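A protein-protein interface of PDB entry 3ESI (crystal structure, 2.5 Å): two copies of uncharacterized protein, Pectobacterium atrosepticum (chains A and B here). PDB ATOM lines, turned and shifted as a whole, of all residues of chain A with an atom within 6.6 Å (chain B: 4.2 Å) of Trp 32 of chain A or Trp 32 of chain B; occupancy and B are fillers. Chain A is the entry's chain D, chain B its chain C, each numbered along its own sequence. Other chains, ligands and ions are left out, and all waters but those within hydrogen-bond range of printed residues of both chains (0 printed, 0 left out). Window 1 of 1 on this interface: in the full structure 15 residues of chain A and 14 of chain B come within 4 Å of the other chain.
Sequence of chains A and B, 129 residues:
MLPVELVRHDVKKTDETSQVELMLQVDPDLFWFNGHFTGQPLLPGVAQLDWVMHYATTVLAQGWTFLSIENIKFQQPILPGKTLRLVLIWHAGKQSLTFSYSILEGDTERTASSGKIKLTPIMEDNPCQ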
ATOM      1  N   MET A   1     -23.408  15.650 -19.585  1.00  0.00           N
ATOM      2  CA  MET A   1     -24.036  14.511 -18.845  1.00  0.00           C
ATOM      3  C   MET A   1     -24.343  14.806 -17.373  1.00  0.00           C
ATOM      4  O   MET A   1     -25.292  14.250 -16.808  1.00  0.00           O
ATOM      5  CB  MET A   1     -23.148  13.256 -18.962  1.00  0.00           C
ATOM      6  CG  MET A   1     -23.134  12.613 -20.358  1.00  0.00           C
ATOM      7  SD  MET A   1     -24.724  11.892 -20.886  1.00  0.00           S
ATOM      8  CE  MET A   1     -24.497  10.250 -20.186  1.00  0.00           C
ATOM      9  N   LEU A   2     -23.561  15.686 -16.753  1.00  0.00           N
ATOM     10  CA  LEU A   2     -23.782  16.019 -15.349  1.00  0.00           C
ATOM     11  C   LEU A   2     -24.622  17.262 -15.170  1.00  0.00           C
ATOM     12  O   LEU A   2     -24.724  18.096 -16.065  1.00  0.00           O
ATOM     13  CB  LEU A   2     -22.451  16.217 -14.624  1.00  0.00           C
ATOM     14  CG  LEU A   2     -21.647  14.931 -14.386  1.00  0.00           C
ATOM     15  CD1 LEU A   2     -20.286  15.284 -13.812  1.00  0.00           C
ATOM     16  CD2 LEU A   2     -22.410  14.009 -13.445  1.00  0.00           C
ATOM     17  N   ASP A  29     -29.583  21.349 -22.326  1.00  0.00           N
ATOM     18  CA  ASP A  29     -28.706  20.854 -23.378  1.00  0.00           C
ATOM     19  C   ASP A  29     -28.051  19.504 -23.108  1.00  0.00           C
ATOM     20  O   ASP A  29     -27.219  19.052 -23.893  1.00  0.00           O
ATOM     21  CB  ASP A  29     -27.633  21.899 -23.701  1.00  0.00           C
ATOM     22  CG  ASP A  29     -28.233  23.227 -24.173  1.00  0.00           C
ATOM     23  OD1 ASP A  29     -29.112  23.204 -25.067  1.00  0.00           O
ATOM     24  OD2 ASP A  29     -27.819  24.296 -23.656  1.00  0.00           O
ATOM     25  N   LEU A  30     -28.423  18.857 -22.008  1.00  0.00           N
ATOM     26  CA  LEU A  30     -27.868  17.544 -21.680  1.00  0.00           C
ATOM     27  C   LEU A  30     -28.281  16.517 -22.738  1.00  0.00           C
ATOM     28  O   LEU A  30     -29.411  16.533 -23.233  1.00  0.00           O
ATOM     29  CB  LEU A  30     -28.373  17.081 -20.314  1.00  0.00           C
ATOM     30  CG  LEU A  30     -28.092  18.010 -19.133  1.00  0.00           C
ATOM     31  CD1 LEU A  30     -28.885  17.529 -17.928  1.00  0.00           C
ATOM     32  CD2 LEU A  30     -26.600  18.065 -18.842  1.00  0.00           C
ATOM     33  N   PHE A  31     -27.364  15.614 -23.070  1.00  0.00           N
ATOM     34  CA  PHE A  31     -27.623  14.576 -24.068  1.00  0.00           C
ATOM     35  C   PHE A  31     -28.879  13.782 -23.747  1.00  0.00           C
ATOM     36  O   PHE A  31     -29.506  13.196 -24.637  1.00  0.00           O
ATOM     37  CB  PHE A  31     -26.420  13.625 -24.173  1.00  0.00           C
ATOM     38  CG  PHE A  31     -25.185  14.267 -24.755  1.00  0.00           C
ATOM     39  CD1 PHE A  31     -25.267  15.047 -25.912  1.00  0.00           C
ATOM     40  CD2 PHE A  31     -23.947  14.084 -24.159  1.00  0.00           C
ATOM     41  CE1 PHE A  31     -24.132  15.639 -26.469  1.00  0.00           C
ATOM     42  CE2 PHE A  31     -22.802  14.669 -24.701  1.00  0.00           C
ATOM     43  CZ  PHE A  31     -22.894  15.452 -25.864  1.00  0.00           C
ATOM     44  N   TRP A  32     -29.244  13.769 -22.467  1.00  0.00           N
ATOM     45  CA  TRP A  32     -30.434  13.056 -22.011  1.00  0.00           C
ATOM     46  C   TRP A  32     -31.693  13.596 -22.687  1.00  0.00           C
ATOM     47  O   TRP A  32     -32.707  12.904 -22.760  1.00  0.00           O
ATOM     48  CB  TRP A  32     -30.600  13.201 -20.493  1.00  0.00           C
ATOM     49  CG  TRP A  32     -29.410  12.761 -19.685  1.00  0.00           C
ATOM     50  CD1 TRP A  32     -28.472  13.562 -19.094  1.00  0.00           C
ATOM     51  CD2 TRP A  32     -29.031  11.412 -19.383  1.00  0.00           C
ATOM     52  NE1 TRP A  32     -27.535  12.793 -18.444  1.00  0.00           N
ATOM     53  CE2 TRP A  32     -27.854  11.471 -18.608  1.00  0.00           C
ATOM     54  CE3 TRP A  32     -29.576  10.158 -19.690  1.00  0.00           C
ATOM     55  CZ2 TRP A  32     -27.213  10.328 -18.137  1.00  0.00           C
ATOM     56  CZ3 TRP A  32     -28.938   9.021 -19.218  1.00  0.00           C
ATOM     57  CH2 TRP A  32     -27.769   9.116 -18.451  1.00  0.00           C
ATOM     58  N   PHE A  33     -31.635  14.829 -23.177  1.00  0.00           N
ATOM     59  CA  PHE A  33     -32.802  15.432 -23.796  1.00  0.00           C
ATOM     60  C   PHE A  33     -32.685  15.649 -25.297  1.00  0.00           C
ATOM     61  O   PHE A  33     -33.553  16.285 -25.903  1.00  0.00           O
ATOM     62  CB  PHE A  33     -33.106  16.774 -23.137  1.00  0.00           C
ATOM     63  CG  PHE A  33     -33.111  16.733 -21.635  1.00  0.00           C
ATOM     64  CD1 PHE A  33     -33.909  15.827 -20.952  1.00  0.00           C
ATOM     65  CD2 PHE A  33     -32.335  17.630 -20.904  1.00  0.00           C
ATOM     66  CE1 PHE A  33     -33.939  15.811 -19.559  1.00  0.00           C
ATOM     67  CE2 PHE A  33     -32.357  17.624 -19.509  1.00  0.00           C
ATOM     68  CZ  PHE A  33     -33.162  16.710 -18.834  1.00  0.00           C
ATOM     69  N   ASN A  34     -31.632  15.125 -25.905  1.00  0.00           N
ATOM     70  CA  ASN A  34     -31.439  15.320 -27.337  1.00  0.00           C
ATOM     71  C   ASN A  34     -32.573  14.799 -28.236  1.00  0.00           C
ATOM     72  O   ASN A  34     -32.897  13.607 -28.247  1.00  0.00           O
ATOM     73  CB  ASN A  34     -30.103  14.712 -27.769  1.00  0.00           C
ATOM     74  CG  ASN A  34     -29.524  15.404 -28.985  1.00  0.00           C
ATOM     75  OD1 ASN A  34     -29.970  15.189 -30.119  1.00  0.00           O
ATOM     76  ND2 ASN A  34     -28.535  16.261 -28.753  1.00  0.00           N
ATOM     77  N   PHE A  37     -32.934  11.393 -29.693  1.00  0.00           N
ATOM     78  CA  PHE A  37     -33.139  10.219 -28.863  1.00  0.00           C
ATOM     79  C   PHE A  37     -34.557  10.107 -28.331  1.00  0.00           C
ATOM     80  O   PHE A  37     -35.197   9.072 -28.484  1.00  0.00           O
ATOM     81  CB  PHE A  37     -32.159  10.217 -27.687  1.00  0.00           C
ATOM     82  CG  PHE A  37     -30.706  10.363 -28.090  1.00  0.00           C
ATOM     83  CD1 PHE A  37     -30.210   9.741 -29.237  1.00  0.00           C
ATOM     84  CD2 PHE A  37     -29.825  11.092 -27.298  1.00  0.00           C
ATOM     85  CE1 PHE A  37     -28.861   9.845 -29.585  1.00  0.00           C
ATOM     86  CE2 PHE A  37     -28.476  11.197 -27.638  1.00  0.00           C
ATOM     87  CZ  PHE A  37     -27.994  10.571 -28.786  1.00  0.00           C
ATOM     88  N   THR A  38     -35.056  11.181 -27.732  1.00  0.00           N
ATOM     89  CA  THR A  38     -36.388  11.167 -27.133  1.00  0.00           C
ATOM     90  C   THR A  38     -37.262  12.352 -27.529  1.00  0.00           C
ATOM     91  O   THR A  38     -36.773  13.470 -27.686  1.00  0.00           O
ATOM     92  CB  THR A  38     -36.263  11.156 -25.591  1.00  0.00           C
ATOM     93  OG1 THR A  38     -37.559  11.078 -24.989  1.00  0.00           O
ATOM     94  CG2 THR A  38     -35.569  12.417 -25.116  1.00  0.00           C
ATOM     95  N   PRO A  41     -38.773  14.473 -23.533  1.00  0.00           N
ATOM     96  CA  PRO A  41     -37.626  14.550 -22.631  1.00  0.00           C
ATOM     97  C   PRO A  41     -37.916  14.647 -21.135  1.00  0.00           C
ATOM     98  O   PRO A  41     -38.758  15.432 -20.683  1.00  0.00           O
ATOM     99  CB  PRO A  41     -36.851  15.758 -23.171  1.00  0.00           C
ATOM    100  CG  PRO A  41     -37.942  16.651 -23.701  1.00  0.00           C
ATOM    101  CD  PRO A  41     -38.869  15.669 -24.395  1.00  0.00           C
ATOM    102  N   LEU A  42     -37.216  13.801 -20.384  1.00  0.00           N
ATOM    103  CA  LEU A  42     -37.291  13.788 -18.931  1.00  0.00           C
ATOM    104  C   LEU A  42     -36.069  13.041 -18.418  1.00  0.00           C
ATOM    105  O   LEU A  42     -35.539  12.164 -19.094  1.00  0.00           O
ATOM    106  CB  LEU A  42     -38.574  13.140 -18.425  1.00  0.00           C
ATOM    107  CG  LEU A  42     -38.794  11.640 -18.550  1.00  0.00           C
ATOM    108  CD1 LEU A  42     -39.635  11.163 -17.356  1.00  0.00           C
ATOM    109  CD2 LEU A  42     -39.473  11.327 -19.875  1.00  0.00           C
ATOM    110  N   LEU A  43     -35.612  13.403 -17.227  1.00  0.00           N
ATOM    111  CA  LEU A  43     -34.437  12.788 -16.638  1.00  0.00           C
ATOM    112  C   LEU A  43     -34.675  11.332 -16.231  1.00  0.00           C
ATOM    113  O   LEU A  43     -35.283  11.060 -15.189  1.00  0.00           O
ATOM    114  CB  LEU A  43     -34.006  13.595 -15.424  1.00  0.00           C
ATOM    115  CG  LEU A  43     -32.524  13.488 -15.098  1.00  0.00           C
ATOM    116  CD1 LEU A  43     -31.737  13.981 -16.304  1.00  0.00           C
ATOM    117  CD2 LEU A  43     -32.198  14.312 -13.857  1.00  0.00           C
ATOM    118  N   PRO A  44     -34.171  10.376 -17.038  1.00  0.00           N
ATOM    119  CA  PRO A  44     -34.332   8.943 -16.766  1.00  0.00           C
ATOM    120  C   PRO A  44     -33.671   8.465 -15.482  1.00  0.00           C
ATOM    121  O   PRO A  44     -32.771   9.116 -14.940  1.00  0.00           O
ATOM    122  CB  PRO A  44     -33.722   8.290 -18.002  1.00  0.00           C
ATOM    123  CG  PRO A  44     -32.617   9.228 -18.349  1.00  0.00           C
ATOM    124  CD  PRO A  44     -33.280  10.590 -18.195  1.00  0.00           C
ATOM    125  N   VAL A  46     -31.504   6.084 -14.913  1.00  0.00           N
ATOM    126  CA  VAL A  46     -30.065   5.857 -14.890  1.00  0.00           C
ATOM    127  C   VAL A  46     -29.327   7.129 -14.513  1.00  0.00           C
ATOM    128  O   VAL A  46     -28.455   7.112 -13.645  1.00  0.00           O
ATOM    129  CB  VAL A  46     -29.525   5.331 -16.246  1.00  0.00           C
ATOM    130  CG1 VAL A  46     -30.173   3.989 -16.561  1.00  0.00           C
ATOM    131  CG2 VAL A  46     -29.810   6.330 -17.356  1.00  0.00           C
ATOM    132  N   ALA A  47     -29.696   8.236 -15.146  1.00  0.00           N
ATOM    133  CA  ALA A  47     -29.048   9.506 -14.867  1.00  0.00           C
ATOM    134  C   ALA A  47     -29.259   9.918 -13.412  1.00  0.00           C
ATOM    135  O   ALA A  47     -28.329  10.377 -12.738  1.00  0.00           O
ATOM    136  CB  ALA A  47     -29.578  10.584 -15.808  1.00  0.00           C
ATOM    137  N   GLN A  48     -30.478   9.752 -12.922  1.00  0.00           N
ATOM    138  CA  GLN A  48     -30.755  10.112 -11.543  1.00  0.00           C
ATOM    139  C   GLN A  48     -29.859   9.307 -10.595  1.00  0.00           C
ATOM    140  O   GLN A  48     -29.335   9.847  -9.616  1.00  0.00           O
ATOM    141  CB  GLN A  48     -32.232   9.886 -11.225  1.00  0.00           C
ATOM    142  CG  GLN A  48     -33.167  10.869 -11.926  1.00  0.00           C
ATOM    143  CD  GLN A  48     -34.622  10.754 -11.461  1.00  0.00           C
ATOM    144  OE1 GLN A  48     -34.897  10.618 -10.269  1.00  0.00           O
ATOM    145  NE2 GLN A  48     -35.551  10.826 -12.401  1.00  0.00           N
ATOM    146  N   ASP A  50     -26.914   7.763 -11.421  1.00  0.00           N
ATOM    147  CA  ASP A  50     -25.538   8.124 -11.692  1.00  0.00           C
ATOM    148  C   ASP A  50     -25.119   9.374 -10.941  1.00  0.00           C
ATOM    149  O   ASP A  50     -24.025   9.417 -10.386  1.00  0.00           O
ATOM    150  CB  ASP A  50     -25.328   8.335 -13.194  1.00  0.00           C
ATOM    151  CG  ASP A  50     -23.952   8.889 -13.515  1.00  0.00           C
ATOM    152  OD1 ASP A  50     -22.951   8.264 -13.124  1.00  0.00           O
ATOM    153  OD2 ASP A  50     -23.868   9.953 -14.152  1.00  0.00           O
ATOM    154  N   TRP A  51     -25.969  10.401 -10.951  1.00  0.00           N
ATOM    155  CA  TRP A  51     -25.669  11.634 -10.240  1.00  0.00           C
ATOM    156  C   TRP A  51     -25.604  11.356  -8.735  1.00  0.00           C
ATOM    157  O   TRP A  51     -24.719  11.866  -8.034  1.00  0.00           O
ATOM    158  CB  TRP A  51     -26.739  12.702 -10.508  1.00  0.00           C
ATOM    159  CG  TRP A  51     -26.814  13.159 -11.929  1.00  0.00           C
ATOM    160  CD1 TRP A  51     -26.048  12.733 -12.964  1.00  0.00           C
ATOM    161  CD2 TRP A  51     -27.718  14.131 -12.470  1.00  0.00           C
ATOM    162  NE1 TRP A  51     -26.412  13.376 -14.122  1.00  0.00           N
ATOM    163  CE2 TRP A  51     -27.435  14.241 -13.849  1.00  0.00           C
ATOM    164  CE3 TRP A  51     -28.742  14.921 -11.921  1.00  0.00           C
ATOM    165  CZ2 TRP A  51     -28.132  15.107 -14.694  1.00  0.00           C
ATOM    166  CZ3 TRP A  51     -29.435  15.781 -12.756  1.00  0.00           C
ATOM    167  CH2 TRP A  51     -29.125  15.869 -14.135  1.00  0.00           C
ATOM    168  N   MET B   1     -21.025   3.029 -15.911  1.00  0.00           N
ATOM    169  CA  MET B   1     -21.399   3.910 -17.060  1.00  0.00           C
ATOM    170  C   MET B   1     -20.526   3.779 -18.320  1.00  0.00           C
ATOM    171  O   MET B   1     -21.045   3.836 -19.447  1.00  0.00           O
ATOM    172  CB  MET B   1     -21.448   5.380 -16.614  1.00  0.00           C
ATOM    173  CG  MET B   1     -22.578   5.717 -15.641  1.00  0.00           C
ATOM    174  SD  MET B   1     -24.271   5.415 -16.257  1.00  0.00           S
ATOM    175  CE  MET B   1     -24.588   7.069 -17.034  1.00  0.00           C
ATOM    176  N   LEU B  30     -23.613  -2.430 -16.253  1.00  0.00           N
ATOM    177  CA  LEU B  30     -23.795  -0.994 -16.435  1.00  0.00           C
ATOM    178  C   LEU B  30     -25.163  -0.534 -15.915  1.00  0.00           C
ATOM    179  O   LEU B  30     -26.140  -1.279 -15.959  1.00  0.00           O
ATOM    180  CB  LEU B  30     -23.665  -0.632 -17.916  1.00  0.00           C
ATOM    181  CG  LEU B  30     -22.277  -0.912 -18.495  1.00  0.00           C
ATOM    182  CD1 LEU B  30     -22.267  -0.687 -20.002  1.00  0.00           C
ATOM    183  CD2 LEU B  30     -21.272  -0.010 -17.796  1.00  0.00           C
ATOM    184  N   PHE B  31     -25.232   0.693 -15.414  1.00  0.00           N
ATOM    185  CA  PHE B  31     -26.497   1.218 -14.906  1.00  0.00           C
ATOM    186  C   PHE B  31     -27.534   1.252 -16.015  1.00  0.00           C
ATOM    187  O   PHE B  31     -28.734   1.173 -15.754  1.00  0.00           O
ATOM    188  CB  PHE B  31     -26.313   2.626 -14.328  1.00  0.00           C
ATOM    189  CG  PHE B  31     -25.554   2.655 -13.026  1.00  0.00           C
ATOM    190  CD1 PHE B  31     -25.733   1.648 -12.075  1.00  0.00           C
ATOM    191  CD2 PHE B  31     -24.706   3.715 -12.722  1.00  0.00           C
ATOM    192  CE1 PHE B  31     -25.087   1.694 -10.847  1.00  0.00           C
ATOM    193  CE2 PHE B  31     -24.053   3.777 -11.496  1.00  0.00           C
ATOM    194  CZ  PHE B  31     -24.244   2.764 -10.553  1.00  0.00           C
ATOM    195  N   TRP B  32     -27.057   1.364 -17.252  1.00  0.00           N
ATOM    196  CA  TRP B  32     -27.929   1.412 -18.417  1.00  0.00           C
ATOM    197  C   TRP B  32     -28.847   0.205 -18.476  1.00  0.00           C
ATOM    198  O   TRP B  32     -29.874   0.241 -19.147  1.00  0.00           O
ATOM    199  CB  TRP B  32     -27.113   1.438 -19.714  1.00  0.00           C
ATOM    200  CG  TRP B  32     -26.043   2.491 -19.771  1.00  0.00           C
ATOM    201  CD1 TRP B  32     -24.698   2.303 -19.642  1.00  0.00           C
ATOM    202  CD2 TRP B  32     -26.237   3.897 -19.965  1.00  0.00           C
ATOM    203  NE1 TRP B  32     -24.041   3.507 -19.744  1.00  0.00           N
ATOM    204  CE2 TRP B  32     -24.962   4.501 -19.940  1.00  0.00           C
ATOM    205  CE3 TRP B  32     -27.364   4.705 -20.154  1.00  0.00           C
ATOM    206  CZ2 TRP B  32     -24.784   5.873 -20.096  1.00  0.00           C
ATOM    207  CZ3 TRP B  32     -27.188   6.070 -20.308  1.00  0.00           C
ATOM    208  CH2 TRP B  32     -25.908   6.642 -20.277  1.00  0.00           C
ATOM    209  N   PHE B  33     -28.485  -0.868 -17.783  1.00  0.00           N
ATOM    210  CA  PHE B  33     -29.294  -2.070 -17.836  1.00  0.00           C
ATOM    211  C   PHE B  33     -29.977  -2.441 -16.542  1.00  0.00           C
ATOM    212  O   PHE B  33     -30.667  -3.460 -16.497  1.00  0.00           O
ATOM    213  CB  PHE B  33     -28.450  -3.268 -18.284  1.00  0.00           C
ATOM    214  CG  PHE B  33     -27.619  -3.009 -19.505  1.00  0.00           C
ATOM    215  CD1 PHE B  33     -28.120  -2.264 -20.564  1.00  0.00           C
ATOM    216  CD2 PHE B  33     -26.326  -3.513 -19.598  1.00  0.00           C
ATOM    217  CE1 PHE B  33     -27.343  -2.021 -21.699  1.00  0.00           C
ATOM    218  CE2 PHE B  33     -25.542  -3.274 -20.730  1.00  0.00           C
ATOM    219  CZ  PHE B  33     -26.055  -2.525 -21.780  1.00  0.00           C
ATOM    220  N   ASN B  34     -29.812  -1.637 -15.494  1.00  0.00           N
ATOM    221  CA  ASN B  34     -30.421  -1.987 -14.214  1.00  0.00           C
ATOM    222  C   ASN B  34     -31.901  -2.360 -14.319  1.00  0.00           C
ATOM    223  O   ASN B  34     -32.709  -1.620 -14.886  1.00  0.00           O
ATOM    224  CB  ASN B  34     -30.232  -0.862 -13.193  1.00  0.00           C
ATOM    225  CG  ASN B  34     -30.468  -1.331 -11.760  1.00  0.00           C
ATOM    226  OD1 ASN B  34     -31.612  -1.507 -11.325  1.00  0.00           O
ATOM    227  ND2 ASN B  34     -29.382  -1.551 -11.025  1.00  0.00           N
ATOM    228  N   LEU B  43     -28.397  -0.741 -24.989  1.00  0.00           N
ATOM    229  CA  LEU B  43     -27.579   0.461 -24.903  1.00  0.00           C
ATOM    230  C   LEU B  43     -28.256   1.593 -25.654  1.00  0.00           C
ATOM    231  O   LEU B  43     -28.298   1.607 -26.881  1.00  0.00           O
ATOM    232  CB  LEU B  43     -26.204   0.179 -25.497  1.00  0.00           C
ATOM    233  CG  LEU B  43     -25.009   1.019 -25.062  1.00  0.00           C
ATOM    234  CD1 LEU B  43     -24.797   0.884 -23.562  1.00  0.00           C
ATOM    235  CD2 LEU B  43     -23.780   0.545 -25.815  1.00  0.00           C
ATOM    236  N   PRO B  44     -28.790   2.571 -24.919  1.00  0.00           N
ATOM    237  CA  PRO B  44     -29.465   3.692 -25.570  1.00  0.00           C
ATOM    238  C   PRO B  44     -28.534   4.638 -26.326  1.00  0.00           C
ATOM    239  O   PRO B  44     -27.309   4.579 -26.178  1.00  0.00           O
ATOM    240  CB  PRO B  44     -30.185   4.369 -24.408  1.00  0.00           C
ATOM    241  CG  PRO B  44     -29.237   4.146 -23.278  1.00  0.00           C
ATOM    242  CD  PRO B  44     -28.826   2.710 -23.451  1.00  0.00           C
ATOM    243  N   VAL B  46     -28.144   7.851 -25.939  1.00  0.00           N
ATOM    244  CA  VAL B  46     -27.401   8.763 -25.087  1.00  0.00           C
ATOM    245  C   VAL B  46     -26.089   8.118 -24.709  1.00  0.00           C
ATOM    246  O   VAL B  46     -25.049   8.781 -24.697  1.00  0.00           O
ATOM    247  CB  VAL B  46     -28.150   9.106 -23.804  1.00  0.00           C
ATOM    248  CG1 VAL B  46     -27.401  10.207 -23.058  1.00  0.00           C
ATOM    249  CG2 VAL B  46     -29.553   9.562 -24.140  1.00  0.00           C
ATOM    250  N   ALA B  47     -26.138   6.823 -24.402  1.00  0.00           N
ATOM    251  CA  ALA B  47     -24.937   6.091 -24.028  1.00  0.00           C
ATOM    252  C   ALA B  47     -23.993   5.952 -25.221  1.00  0.00           C
ATOM    253  O   ALA B  47     -22.796   6.212 -25.106  1.00  0.00           O
ATOM    254  CB  ALA B  47     -25.309   4.711 -23.454  1.00  0.00           C
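Met 1 of chain A touches Trp 32 of chain B, but with the chains exchanged Trp 32 of chain A does not touch Met 1 of chain B (4.04 Å). Met 1 of chain A touches Val 46 of chain B, but with the chains exchanged Val 46 of chain A does not touch Met 1 of chain B (5.1 Å). Trp 32 of chain B touches its own counterpart, Trp 32 of chain A. Val 46 of chain A touches Trp 32 of chain B, but with the chains exchanged Trp 32 of chain A does not touch Val 46 of chain B (4.01 Å). 10 positions are printed for both chains. Of the 8 pairs that touch across the chains among the printed residues, 3 have their exchanged pair printed and touching as well.
Of chain A, only Met 1, Trp 32 and Val 46 come within 4 Å of Trp 32 of chain B. Of the printed residues of chain B, Val 46 of chain A touches Phe 31 (3.3 Å) and Trp 32 (3.9 Å). Of the printed residues of chain B, Phe 31 of chain A touches Val 46 (3.7 Å). Of the printed residues of chain B, Asp 50 of chain A touches Met 1 (3.6 Å). Of the printed residues of chain A, Val 46 of chain B touches Met 1, Phe 31 and Phe 37. Of the printed residues of chain B, Phe 37 of chain A touches Val 46 (3.5 Å). Trp 51 of chain A touches none of the printed residues of chain B. Leu 30 of chain A touches none of the printed residues of chain B. The nearest printed residue of chain B that does not touch Trp 32 of chain A is Val 46 of chain B (4.01 Å). The nearest residue of chain A that does not touch Trp 32 of chain B is Ala 47 of chain A (6.1 Å). The nearest printed residue of chain A that does not touch Met 1 of chain B is Trp 32 of chain A (4.04 Å).
The backbone carbonyl oxygen (O) of Met 1 of chain A is in hydrogen-bond range of the indole nitrogen (NE1) of Trp 51 of chain A (3.0 Å). O of Met 1 of chain B is in hydrogen-bond range of NE1 of Trp 32 of chain B (3.0 Å). O of Met 1 of chain A is in hydrogen-bond range of NE1 of Trp 32 of chain A (3.1 Å).
CH2 of Trp 32 of chain B touches CE of Met 1 of chain A, at 3.9 Å. Val 46 of chain B touches Met 1 of chain A. CG2 of Val 46 of chain B touches O of Phe 31 of chain A (3.7 Å). CH2 of Trp 32 of chain B touches CH2 of Trp 32 of chain A, at 3.6 Å. Phe 37 of chain A touches Val 46 of chain B. CG1 of Val 46 of chain A touches O of Phe 31 of chain B (3.3 Å). CG1 of Val 46 of chain A touches CA of Trp 32 of chain B, at 3.9 Å. Met 1 of chain B touches Asp 50 of chain A (CG to OD1, 3.6 Å).
Along chain A the printed residues that touch a printed residue of chain B span positions 1 to 50. Printed residues of chain B that touch a printed residue of chain A: Met 1, Phe 31, Trp 32 and Val 46. Among the printed residues, 8 pairs touch across the chains. Among the printed residues, no Asp or Glu carboxylate lies within 4 Å of a Lys or Arg side-chain nitrogen of the other chain.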
